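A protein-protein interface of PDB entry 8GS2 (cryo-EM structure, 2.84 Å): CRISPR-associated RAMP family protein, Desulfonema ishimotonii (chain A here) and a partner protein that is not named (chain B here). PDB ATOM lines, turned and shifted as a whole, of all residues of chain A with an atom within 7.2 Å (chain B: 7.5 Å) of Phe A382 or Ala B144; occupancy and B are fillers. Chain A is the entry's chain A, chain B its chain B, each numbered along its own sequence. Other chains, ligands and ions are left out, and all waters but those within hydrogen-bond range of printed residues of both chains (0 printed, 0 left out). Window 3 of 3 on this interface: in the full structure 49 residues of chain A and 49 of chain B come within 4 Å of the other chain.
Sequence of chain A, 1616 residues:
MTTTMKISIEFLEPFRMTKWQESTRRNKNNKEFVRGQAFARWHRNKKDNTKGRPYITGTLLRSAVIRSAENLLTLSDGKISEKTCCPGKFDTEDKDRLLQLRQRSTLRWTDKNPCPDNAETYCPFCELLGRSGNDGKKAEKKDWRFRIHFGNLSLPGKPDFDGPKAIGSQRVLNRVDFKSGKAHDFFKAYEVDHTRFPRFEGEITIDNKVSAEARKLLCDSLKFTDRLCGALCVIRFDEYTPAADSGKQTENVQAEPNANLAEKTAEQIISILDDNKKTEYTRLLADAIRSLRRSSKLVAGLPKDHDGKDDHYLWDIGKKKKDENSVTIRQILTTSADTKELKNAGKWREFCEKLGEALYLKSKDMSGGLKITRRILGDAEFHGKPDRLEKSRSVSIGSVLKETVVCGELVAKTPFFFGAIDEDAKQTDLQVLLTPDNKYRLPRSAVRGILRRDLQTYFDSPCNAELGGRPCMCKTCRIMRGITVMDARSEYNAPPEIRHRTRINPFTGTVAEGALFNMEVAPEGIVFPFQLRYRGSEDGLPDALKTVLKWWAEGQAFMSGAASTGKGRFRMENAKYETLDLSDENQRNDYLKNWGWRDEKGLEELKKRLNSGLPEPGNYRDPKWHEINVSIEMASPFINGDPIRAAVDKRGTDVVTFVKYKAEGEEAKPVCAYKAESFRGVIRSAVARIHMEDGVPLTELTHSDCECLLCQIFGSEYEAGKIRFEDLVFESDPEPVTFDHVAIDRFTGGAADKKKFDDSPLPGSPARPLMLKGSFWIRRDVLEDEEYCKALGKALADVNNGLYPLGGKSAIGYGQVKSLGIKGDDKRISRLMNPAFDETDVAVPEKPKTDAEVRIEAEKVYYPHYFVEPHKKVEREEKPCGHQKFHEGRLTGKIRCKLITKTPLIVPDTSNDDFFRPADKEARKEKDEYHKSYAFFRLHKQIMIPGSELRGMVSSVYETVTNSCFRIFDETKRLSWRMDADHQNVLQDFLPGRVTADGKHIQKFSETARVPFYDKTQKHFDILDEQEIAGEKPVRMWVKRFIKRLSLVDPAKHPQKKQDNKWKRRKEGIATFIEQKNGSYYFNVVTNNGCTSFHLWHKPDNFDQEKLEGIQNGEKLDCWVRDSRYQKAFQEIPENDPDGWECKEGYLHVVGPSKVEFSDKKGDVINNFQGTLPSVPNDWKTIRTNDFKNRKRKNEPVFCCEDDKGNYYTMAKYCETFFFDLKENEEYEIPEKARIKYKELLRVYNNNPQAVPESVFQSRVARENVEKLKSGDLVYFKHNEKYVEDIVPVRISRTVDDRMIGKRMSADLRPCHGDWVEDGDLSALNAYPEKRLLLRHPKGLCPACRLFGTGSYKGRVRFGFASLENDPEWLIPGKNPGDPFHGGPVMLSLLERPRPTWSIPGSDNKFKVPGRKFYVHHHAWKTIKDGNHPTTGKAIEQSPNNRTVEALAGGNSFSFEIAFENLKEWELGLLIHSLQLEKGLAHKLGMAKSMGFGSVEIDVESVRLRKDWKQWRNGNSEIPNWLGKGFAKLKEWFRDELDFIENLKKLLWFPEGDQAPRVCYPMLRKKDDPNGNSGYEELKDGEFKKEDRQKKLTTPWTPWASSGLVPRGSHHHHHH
Among the printed residues, pairs that only touch across the chains: Leu A377 with Tyr B135, Leu A377 with Arg B145, Leu A377 with Glu B148, Leu A377 with Ala B149, Gly A378 with Arg B145, Ala A380 with Glu B148 and Phe A382 with Ala B144.
Of the 19 printed residues of chain A, 4 touch a printed residue of chain B. Hydrophobic or aromatic side chains of chain A within 4 Å of the printed part of chain B: Leu A377, Ala A380 and Phe A382. Hydrophobic or aromatic side chains of chain B within 4 Å of the printed part of chain A: Tyr B135, Ala B144 and Ala B149.
O of Phe A186 lies within hydrogen-bond range of N of Phe A382 (2.8 Å).
Phe A382 touches one residue of chain B. Of chain A, only Phe A382 comes within 4 Å of Ala B144. Printed residues of chain B within 4 Å of Ala A380: Glu B148 (3.8 Å). Of the printed residues of chain B, Leu A377 touches Tyr B135, Arg B145, Glu B148 and Ala B149. Of the printed residues of chain A, Ala B149 touches Leu A377 (3.8 Å). Ser B141 touches none of the printed residues of chain A. Arg A35 touches none of the printed residues of chain B.
OE1 of Glu B148 sits at hydrogen-bond distance from N of Gly A378, at 2.9 Å.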
ATOM      1  N   LYS A  31      12.012  32.520 -11.044  1.00  0.00           N
ATOM      2  CA  LYS A  31      12.929  31.395 -10.891  1.00  0.00           C
ATOM      3  C   LYS A  31      14.382  31.856 -10.881  1.00  0.00           C
ATOM      4  O   LYS A  31      15.194  31.348 -10.100  1.00  0.00           O
ATOM      5  CB  LYS A  31      12.699  30.373 -12.004  1.00  0.00           C
ATOM      6  CG  LYS A  31      11.321  29.736 -11.984  1.00  0.00           C
ATOM      7  CD  LYS A  31      11.197  28.667 -13.053  1.00  0.00           C
ATOM      8  CE  LYS A  31      12.227  27.572 -12.849  1.00  0.00           C
ATOM      9  NZ  LYS A  31      12.160  26.529 -13.909  1.00  0.00           N
ATOM     10  N   ARG A  35      17.070  31.337  -7.886  1.00  0.00           N
ATOM     11  CA  ARG A  35      18.251  30.536  -8.193  1.00  0.00           C
ATOM     12  C   ARG A  35      19.530  31.237  -7.749  1.00  0.00           C
ATOM     13  O   ARG A  35      20.454  30.593  -7.239  1.00  0.00           O
ATOM     14  CB  ARG A  35      18.292  30.232  -9.690  1.00  0.00           C
ATOM     15  CG  ARG A  35      19.518  29.463 -10.139  1.00  0.00           C
ATOM     16  CD  ARG A  35      19.636  28.145  -9.406  1.00  0.00           C
ATOM     17  NE  ARG A  35      20.854  27.429  -9.763  1.00  0.00           N
ATOM     18  CZ  ARG A  35      22.039  27.646  -9.211  1.00  0.00           C
ATOM     19  NH1 ARG A  35      22.210  28.575  -8.286  1.00  0.00           N
ATOM     20  NH2 ARG A  35      23.079  26.916  -9.600  1.00  0.00           N
ATOM     21  N   LEU A 173      26.992  27.497 -17.694  1.00  0.00           N
ATOM     22  CA  LEU A 173      27.207  26.238 -16.992  1.00  0.00           C
ATOM     23  C   LEU A 173      26.062  25.301 -17.346  1.00  0.00           C
ATOM     24  O   LEU A 173      24.895  25.641 -17.135  1.00  0.00           O
ATOM     25  CB  LEU A 173      27.275  26.461 -15.482  1.00  0.00           C
ATOM     26  CG  LEU A 173      28.089  27.674 -15.035  1.00  0.00           C
ATOM     27  CD1 LEU A 173      27.831  27.987 -13.577  1.00  0.00           C
ATOM     28  CD2 LEU A 173      29.563  27.435 -15.272  1.00  0.00           C
ATOM     29  N   ARG A 175      24.257  21.165 -17.732  1.00  0.00           N
ATOM     30  CA  ARG A 175      24.018  19.919 -17.019  1.00  0.00           C
ATOM     31  C   ARG A 175      24.031  18.788 -18.035  1.00  0.00           C
ATOM     32  O   ARG A 175      23.161  18.728 -18.910  1.00  0.00           O
ATOM     33  CB  ARG A 175      22.690  19.965 -16.262  1.00  0.00           C
ATOM     34  CG  ARG A 175      22.391  18.729 -15.438  1.00  0.00           C
ATOM     35  CD  ARG A 175      21.308  19.014 -14.414  1.00  0.00           C
ATOM     36  NE  ARG A 175      20.121  19.599 -15.027  1.00  0.00           N
ATOM     37  CZ  ARG A 175      19.011  18.927 -15.303  1.00  0.00           C
ATOM     38  NH1 ARG A 175      18.892  17.642 -15.017  1.00  0.00           N
ATOM     39  NH2 ARG A 175      17.994  19.564 -15.876  1.00  0.00           N
ATOM     40  N   HIS A 184      21.977  18.335 -21.130  1.00  0.00           N
ATOM     41  CA  HIS A 184      20.519  18.384 -21.137  1.00  0.00           C
ATOM     42  C   HIS A 184      20.009  19.819 -21.207  1.00  0.00           C
ATOM     43  O   HIS A 184      19.081  20.120 -21.966  1.00  0.00           O
ATOM     44  CB  HIS A 184      19.972  17.673 -19.897  1.00  0.00           C
ATOM     45  CG  HIS A 184      18.477  17.635 -19.829  1.00  0.00           C
ATOM     46  ND1 HIS A 184      17.762  18.253 -18.828  1.00  0.00           N
ATOM     47  CD2 HIS A 184      17.562  17.050 -20.638  1.00  0.00           C
ATOM     48  CE1 HIS A 184      16.471  18.052 -19.022  1.00  0.00           C
ATOM     49  NE2 HIS A 184      16.323  17.325 -20.114  1.00  0.00           N
ATOM     50  N   ASP A 185      20.607  20.715 -20.429  1.00  0.00           N
ATOM     51  CA  ASP A 185      20.236  22.125 -20.407  1.00  0.00           C
ATOM     52  C   ASP A 185      21.425  22.912 -19.867  1.00  0.00           C
ATOM     53  O   ASP A 185      22.531  22.378 -19.737  1.00  0.00           O
ATOM     54  CB  ASP A 185      18.961  22.342 -19.585  1.00  0.00           C
ATOM     55  CG  ASP A 185      18.985  21.604 -18.265  1.00  0.00           C
ATOM     56  OD1 ASP A 185      20.061  21.110 -17.878  1.00  0.00           O
ATOM     57  OD2 ASP A 185      17.923  21.508 -17.618  1.00  0.00           O
ATOM     58  N   PHE A 186      21.204  24.186 -19.550  1.00  0.00           N
ATOM     59  CA  PHE A 186      22.291  25.039 -19.089  1.00  0.00           C
ATOM     60  C   PHE A 186      21.723  26.225 -18.323  1.00  0.00           C
ATOM     61  O   PHE A 186      20.516  26.476 -18.327  1.00  0.00           O
ATOM     62  CB  PHE A 186      23.159  25.517 -20.260  1.00  0.00           C
ATOM     63  CG  PHE A 186      22.444  26.434 -21.213  1.00  0.00           C
ATOM     64  CD1 PHE A 186      21.669  25.921 -22.238  1.00  0.00           C
ATOM     65  CD2 PHE A 186      22.552  27.808 -21.088  1.00  0.00           C
ATOM     66  CE1 PHE A 186      21.015  26.761 -23.113  1.00  0.00           C
ATOM     67  CE2 PHE A 186      21.901  28.650 -21.960  1.00  0.00           C
ATOM     68  CZ  PHE A 186      21.132  28.125 -22.974  1.00  0.00           C
ATOM     69  N   PHE A 187      22.621  26.947 -17.655  1.00  0.00           N
ATOM     70  CA  PHE A 187      22.295  28.208 -17.008  1.00  0.00           C
ATOM     71  C   PHE A 187      23.560  29.052 -16.948  1.00  0.00           C
ATOM     72  O   PHE A 187      24.674  28.543 -17.096  1.00  0.00           O
ATOM     73  CB  PHE A 187      21.699  28.000 -15.609  1.00  0.00           C
ATOM     74  CG  PHE A 187      22.705  27.609 -14.563  1.00  0.00           C
ATOM     75  CD1 PHE A 187      23.303  26.360 -14.585  1.00  0.00           C
ATOM     76  CD2 PHE A 187      23.035  28.482 -13.543  1.00  0.00           C
ATOM     77  CE1 PHE A 187      24.222  26.000 -13.621  1.00  0.00           C
ATOM     78  CE2 PHE A 187      23.953  28.124 -12.576  1.00  0.00           C
ATOM     79  CZ  PHE A 187      24.545  26.882 -12.616  1.00  0.00           C
ATOM     80  N   LYS A 188      23.379  30.352 -16.739  1.00  0.00           N
ATOM     81  CA  LYS A 188      24.479  31.304 -16.753  1.00  0.00           C
ATOM     82  C   LYS A 188      24.647  31.950 -15.386  1.00  0.00           C
ATOM     83  O   LYS A 188      23.698  32.045 -14.602  1.00  0.00           O
ATOM     84  CB  LYS A 188      24.259  32.400 -17.801  1.00  0.00           C
ATOM     85  CG  LYS A 188      24.158  31.906 -19.229  1.00  0.00           C
ATOM     86  CD  LYS A 188      24.086  33.078 -20.189  1.00  0.00           C
ATOM     87  CE  LYS A 188      23.868  32.619 -21.617  1.00  0.00           C
ATOM     88  NZ  LYS A 188      23.784  33.770 -22.557  1.00  0.00           N
ATOM     89  N   LEU A 377      14.716  26.194 -30.731  1.00  0.00           N
ATOM     90  CA  LEU A 377      14.278  25.948 -29.367  1.00  0.00           C
ATOM     91  C   LEU A 377      15.407  25.280 -28.598  1.00  0.00           C
ATOM     92  O   LEU A 377      16.209  24.536 -29.166  1.00  0.00           O
ATOM     93  CB  LEU A 377      13.021  25.067 -29.318  1.00  0.00           C
ATOM     94  CG  LEU A 377      11.702  25.687 -29.778  1.00  0.00           C
ATOM     95  CD1 LEU A 377      10.604  24.642 -29.797  1.00  0.00           C
ATOM     96  CD2 LEU A 377      11.319  26.848 -28.879  1.00  0.00           C
ATOM     97  N   GLY A 378      15.457  25.551 -27.300  1.00  0.00           N
ATOM     98  CA  GLY A 378      16.456  24.965 -26.436  1.00  0.00           C
ATOM     99  C   GLY A 378      17.632  25.849 -26.091  1.00  0.00           C
ATOM    100  O   GLY A 378      18.544  25.387 -25.399  1.00  0.00           O
ATOM    101  N   ALA A 380      17.509  28.549 -24.169  1.00  0.00           N
ATOM    102  CA  ALA A 380      17.108  29.339 -23.016  1.00  0.00           C
ATOM    103  C   ALA A 380      17.588  28.654 -21.746  1.00  0.00           C
ATOM    104  O   ALA A 380      17.587  27.423 -21.656  1.00  0.00           O
ATOM    105  CB  ALA A 380      15.589  29.526 -22.970  1.00  0.00           C
ATOM    106  N   GLU A 381      18.008  29.456 -20.772  1.00  0.00           N
ATOM    107  CA  GLU A 381      18.530  28.914 -19.528  1.00  0.00           C
ATOM    108  C   GLU A 381      17.432  28.210 -18.739  1.00  0.00           C
ATOM    109  O   GLU A 381      16.271  28.627 -18.737  1.00  0.00           O
ATOM    110  CB  GLU A 381      19.142  30.024 -18.676  1.00  0.00           C
ATOM    111  CG  GLU A 381      20.126  30.905 -19.415  1.00  0.00           C
ATOM    112  CD  GLU A 381      20.575  32.087 -18.582  1.00  0.00           C
ATOM    113  OE1 GLU A 381      20.505  31.999 -17.339  1.00  0.00           O
ATOM    114  OE2 GLU A 381      20.989  33.108 -19.170  1.00  0.00           O
ATOM    115  N   PHE A 382      17.814  27.131 -18.064  1.00  0.00           N
ATOM    116  CA  PHE A 382      16.922  26.401 -17.173  1.00  0.00           C
ATOM    117  C   PHE A 382      17.444  26.541 -15.751  1.00  0.00           C
ATOM    118  O   PHE A 382      18.613  26.244 -15.484  1.00  0.00           O
ATOM    119  CB  PHE A 382      16.822  24.929 -17.569  1.00  0.00           C
ATOM    120  CG  PHE A 382      15.878  24.137 -16.711  1.00  0.00           C
ATOM    121  CD1 PHE A 382      14.519  24.136 -16.974  1.00  0.00           C
ATOM    122  CD2 PHE A 382      16.347  23.396 -15.641  1.00  0.00           C
ATOM    123  CE1 PHE A 382      13.649  23.412 -16.187  1.00  0.00           C
ATOM    124  CE2 PHE A 382      15.482  22.670 -14.851  1.00  0.00           C
ATOM    125  CZ  PHE A 382      14.131  22.679 -15.124  1.00  0.00           C
ATOM    126  N   HIS A 383      16.579  26.984 -14.846  1.00  0.00           N
ATOM    127  CA  HIS A 383      16.932  27.197 -13.453  1.00  0.00           C
ATOM    128  C   HIS A 383      16.194  26.197 -12.575  1.00  0.00           C
ATOM    129  O   HIS A 383      15.008  25.930 -12.787  1.00  0.00           O
ATOM    130  CB  HIS A 383      16.597  28.624 -13.014  1.00  0.00           C
ATOM    131  CG  HIS A 383      17.364  29.677 -13.752  1.00  0.00           C
ATOM    132  ND1 HIS A 383      16.755  30.749 -14.365  1.00  0.00           N
ATOM    133  CD2 HIS A 383      18.692  29.822 -13.973  1.00  0.00           C
ATOM    134  CE1 HIS A 383      17.674  31.508 -14.934  1.00  0.00           C
ATOM    135  NE2 HIS A 383      18.857  30.968 -14.710  1.00  0.00           N
ATOM    136  N   GLY A 384      16.906  25.636 -11.602  1.00  0.00           N
ATOM    137  CA  GLY A 384      16.270  24.709 -10.683  1.00  0.00           C
ATOM    138  C   GLY A 384      15.205  25.402  -9.852  1.00  0.00           C
ATOM    139  O   GLY A 384      15.392  26.521  -9.370  1.00  0.00           O
ATOM    140  N   LYS A 385      14.070  24.728  -9.692  1.00  0.00           N
ATOM    141  CA  LYS A 385      12.959  25.276  -8.927  1.00  0.00           C
ATOM    142  C   LYS A 385      12.843  24.544  -7.599  1.00  0.00           C
ATOM    143  O   LYS A 385      12.454  23.365  -7.582  1.00  0.00           O
ATOM    144  CB  LYS A 385      11.652  25.167  -9.713  1.00  0.00           C
ATOM    145  CG  LYS A 385      10.498  25.929  -9.087  1.00  0.00           C
ATOM    146  CD  LYS A 385       9.214  25.734  -9.870  1.00  0.00           C
ATOM    147  CE  LYS A 385       8.103  26.614  -9.320  1.00  0.00           C
ATOM    148  NZ  LYS A 385       7.859  26.362  -7.873  1.00  0.00           N
ATOM    149  N   GLU A 466      16.340  15.255 -10.309  1.00  0.00           N
ATOM    150  CA  GLU A 466      15.984  16.524 -10.921  1.00  0.00           C
ATOM    151  C   GLU A 466      16.269  17.658  -9.945  1.00  0.00           C
ATOM    152  O   GLU A 466      16.232  17.472  -8.726  1.00  0.00           O
ATOM    153  CB  GLU A 466      14.506  16.538 -11.343  1.00  0.00           C
ATOM    154  CG  GLU A 466      14.077  17.766 -12.134  1.00  0.00           C
ATOM    155  CD  GLU A 466      14.805  17.903 -13.459  1.00  0.00           C
ATOM    156  OE1 GLU A 466      15.226  16.870 -14.021  1.00  0.00           O
ATOM    157  OE2 GLU A 466      14.958  19.047 -13.937  1.00  0.00           O
ATOM    158  N   LEU A 467      16.572  18.830 -10.496  1.00  0.00           N
ATOM    159  CA  LEU A 467      16.854  19.999  -9.674  1.00  0.00           C
ATOM    160  C   LEU A 467      15.646  20.359  -8.820  1.00  0.00           C
ATOM    161  O   LEU A 467      14.504  20.338  -9.285  1.00  0.00           O
ATOM    162  CB  LEU A 467      17.241  21.181 -10.559  1.00  0.00           C
ATOM    163  CG  LEU A 467      18.438  20.966 -11.482  1.00  0.00           C
ATOM    164  CD1 LEU A 467      18.554  22.111 -12.466  1.00  0.00           C
ATOM    165  CD2 LEU A 467      19.711  20.825 -10.672  1.00  0.00           C
ATOM    166  N   TYR B 135       4.514  19.519 -27.776  1.00  0.00           N
ATOM    167  CA  TYR B 135       5.174  18.907 -26.630  1.00  0.00           C
ATOM    168  C   TYR B 135       4.134  18.270 -25.716  1.00  0.00           C
ATOM    169  O   TYR B 135       3.303  18.971 -25.128  1.00  0.00           O
ATOM    170  CB  TYR B 135       5.996  19.943 -25.869  1.00  0.00           C
ATOM    171  CG  TYR B 135       7.248  20.383 -26.590  1.00  0.00           C
ATOM    172  CD1 TYR B 135       8.392  19.596 -26.575  1.00  0.00           C
ATOM    173  CD2 TYR B 135       7.291  21.586 -27.280  1.00  0.00           C
ATOM    174  CE1 TYR B 135       9.538  19.992 -27.230  1.00  0.00           C
ATOM    175  CE2 TYR B 135       8.435  21.992 -27.938  1.00  0.00           C
ATOM    176  CZ  TYR B 135       9.555  21.190 -27.909  1.00  0.00           C
ATOM    177  OH  TYR B 135      10.698  21.588 -28.562  1.00  0.00           O
ATOM    178  N   SER B 141       6.592  17.113 -14.410  1.00  0.00           N
ATOM    179  CA  SER B 141       7.492  18.139 -14.921  1.00  0.00           C
ATOM    180  C   SER B 141       7.044  18.590 -16.307  1.00  0.00           C
ATOM    181  O   SER B 141       7.027  17.795 -17.252  1.00  0.00           O
ATOM    182  CB  SER B 141       8.921  17.608 -14.968  1.00  0.00           C
ATOM    183  OG  SER B 141       9.014  16.477 -15.816  1.00  0.00           O
ATOM    184  N   VAL B 142       6.684  19.861 -16.425  1.00  0.00           N
ATOM    185  CA  VAL B 142       6.333  20.431 -17.730  1.00  0.00           C
ATOM    186  C   VAL B 142       7.595  20.556 -18.575  1.00  0.00           C
ATOM    187  O   VAL B 142       8.663  20.895 -18.033  1.00  0.00           O
ATOM    188  CB  VAL B 142       5.646  21.788 -17.547  1.00  0.00           C
ATOM    189  CG1 VAL B 142       6.470  22.685 -16.635  1.00  0.00           C
ATOM    190  CG2 VAL B 142       5.406  22.464 -18.888  1.00  0.00           C
ATOM    191  N   PRO B 143       7.545  20.264 -19.876  1.00  0.00           N
ATOM    192  CA  PRO B 143       8.725  20.485 -20.720  1.00  0.00           C
ATOM    193  C   PRO B 143       9.149  21.947 -20.698  1.00  0.00           C
ATOM    194  O   PRO B 143       8.316  22.855 -20.693  1.00  0.00           O
ATOM    195  CB  PRO B 143       8.250  20.057 -22.112  1.00  0.00           C
ATOM    196  CG  PRO B 143       7.155  19.088 -21.848  1.00  0.00           C
ATOM    197  CD  PRO B 143       6.466  19.577 -20.608  1.00  0.00           C
ATOM    198  N   ALA B 144      10.463  22.165 -20.681  1.00  0.00           N
ATOM    199  CA  ALA B 144      11.003  23.515 -20.618  1.00  0.00           C
ATOM    200  C   ALA B 144      11.026  24.211 -21.971  1.00  0.00           C
ATOM    201  O   ALA B 144      11.206  25.433 -22.013  1.00  0.00           O
ATOM    202  CB  ALA B 144      12.415  23.490 -20.032  1.00  0.00           C
ATOM    203  N   ARG B 145      10.850  23.477 -23.069  1.00  0.00           N
ATOM    204  CA  ARG B 145      10.836  24.083 -24.392  1.00  0.00           C
ATOM    205  C   ARG B 145       9.447  24.496 -24.851  1.00  0.00           C
ATOM    206  O   ARG B 145       9.336  25.319 -25.764  1.00  0.00           O
ATOM    207  CB  ARG B 145      11.449  23.128 -25.422  1.00  0.00           C
ATOM    208  CG  ARG B 145      12.916  22.835 -25.172  1.00  0.00           C
ATOM    209  CD  ARG B 145      13.533  22.053 -26.311  1.00  0.00           C
ATOM    210  NE  ARG B 145      14.940  21.767 -26.062  1.00  0.00           N
ATOM    211  CZ  ARG B 145      15.739  21.140 -26.914  1.00  0.00           C
ATOM    212  NH1 ARG B 145      15.303  20.721 -28.090  1.00  0.00           N
ATOM    213  NH2 ARG B 145      17.007  20.927 -26.577  1.00  0.00           N
ATOM    214  N   LYS B 146       8.390  23.943 -24.251  1.00  0.00           N
ATOM    215  CA  LYS B 146       7.052  24.457 -24.513  1.00  0.00           C
ATOM    216  C   LYS B 146       6.896  25.869 -23.967  1.00  0.00           C
ATOM    217  O   LYS B 146       6.296  26.731 -24.618  1.00  0.00           O
ATOM    218  CB  LYS B 146       5.999  23.529 -23.909  1.00  0.00           C
ATOM    219  CG  LYS B 146       4.575  24.039 -24.055  1.00  0.00           C
ATOM    220  CD  LYS B 146       3.563  23.032 -23.538  1.00  0.00           C
ATOM    221  CE  LYS B 146       2.145  23.554 -23.689  1.00  0.00           C
ATOM    222  NZ  LYS B 146       1.138  22.581 -23.188  1.00  0.00           N
ATOM    223  N   VAL B 147       7.431  26.121 -22.769  1.00  0.00           N
ATOM    224  CA  VAL B 147       7.398  27.464 -22.199  1.00  0.00           C
ATOM    225  C   VAL B 147       8.200  28.426 -23.062  1.00  0.00           C
ATOM    226  O   VAL B 147       7.781  29.564 -23.306  1.00  0.00           O
ATOM    227  CB  VAL B 147       7.914  27.439 -20.749  1.00  0.00           C
ATOM    228  CG1 VAL B 147       7.891  28.836 -20.154  1.00  0.00           C
ATOM    229  CG2 VAL B 147       7.088  26.481 -19.910  1.00  0.00           C
ATOM    230  N   GLU B 148       9.370  27.988 -23.531  1.00  0.00           N
ATOM    231  CA  GLU B 148      10.197  28.839 -24.377  1.00  0.00           C
ATOM    232  C   GLU B 148       9.493  29.170 -25.687  1.00  0.00           C
ATOM    233  O   GLU B 148       9.572  30.305 -26.172  1.00  0.00           O
ATOM    234  CB  GLU B 148      11.537  28.158 -24.646  1.00  0.00           C
ATOM    235  CG  GLU B 148      12.432  28.920 -25.598  1.00  0.00           C
ATOM    236  CD  GLU B 148      13.693  28.159 -25.938  1.00  0.00           C
ATOM    237  OE1 GLU B 148      13.934  27.101 -25.320  1.00  0.00           O
ATOM    238  OE2 GLU B 148      14.441  28.616 -26.824  1.00  0.00           O
ATOM    239  N   ALA B 149       8.810  28.189 -26.280  1.00  0.00           N
ATOM    240  CA  ALA B 149       8.102  28.434 -27.533  1.00  0.00           C
ATOM    241  C   ALA B 149       6.977  29.443 -27.350  1.00  0.00           C
ATOM    242  O   ALA B 149       6.788  30.328 -28.192  1.00  0.00           O
ATOM    243  CB  ALA B 149       7.561  27.121 -28.094  1.00  0.00           C
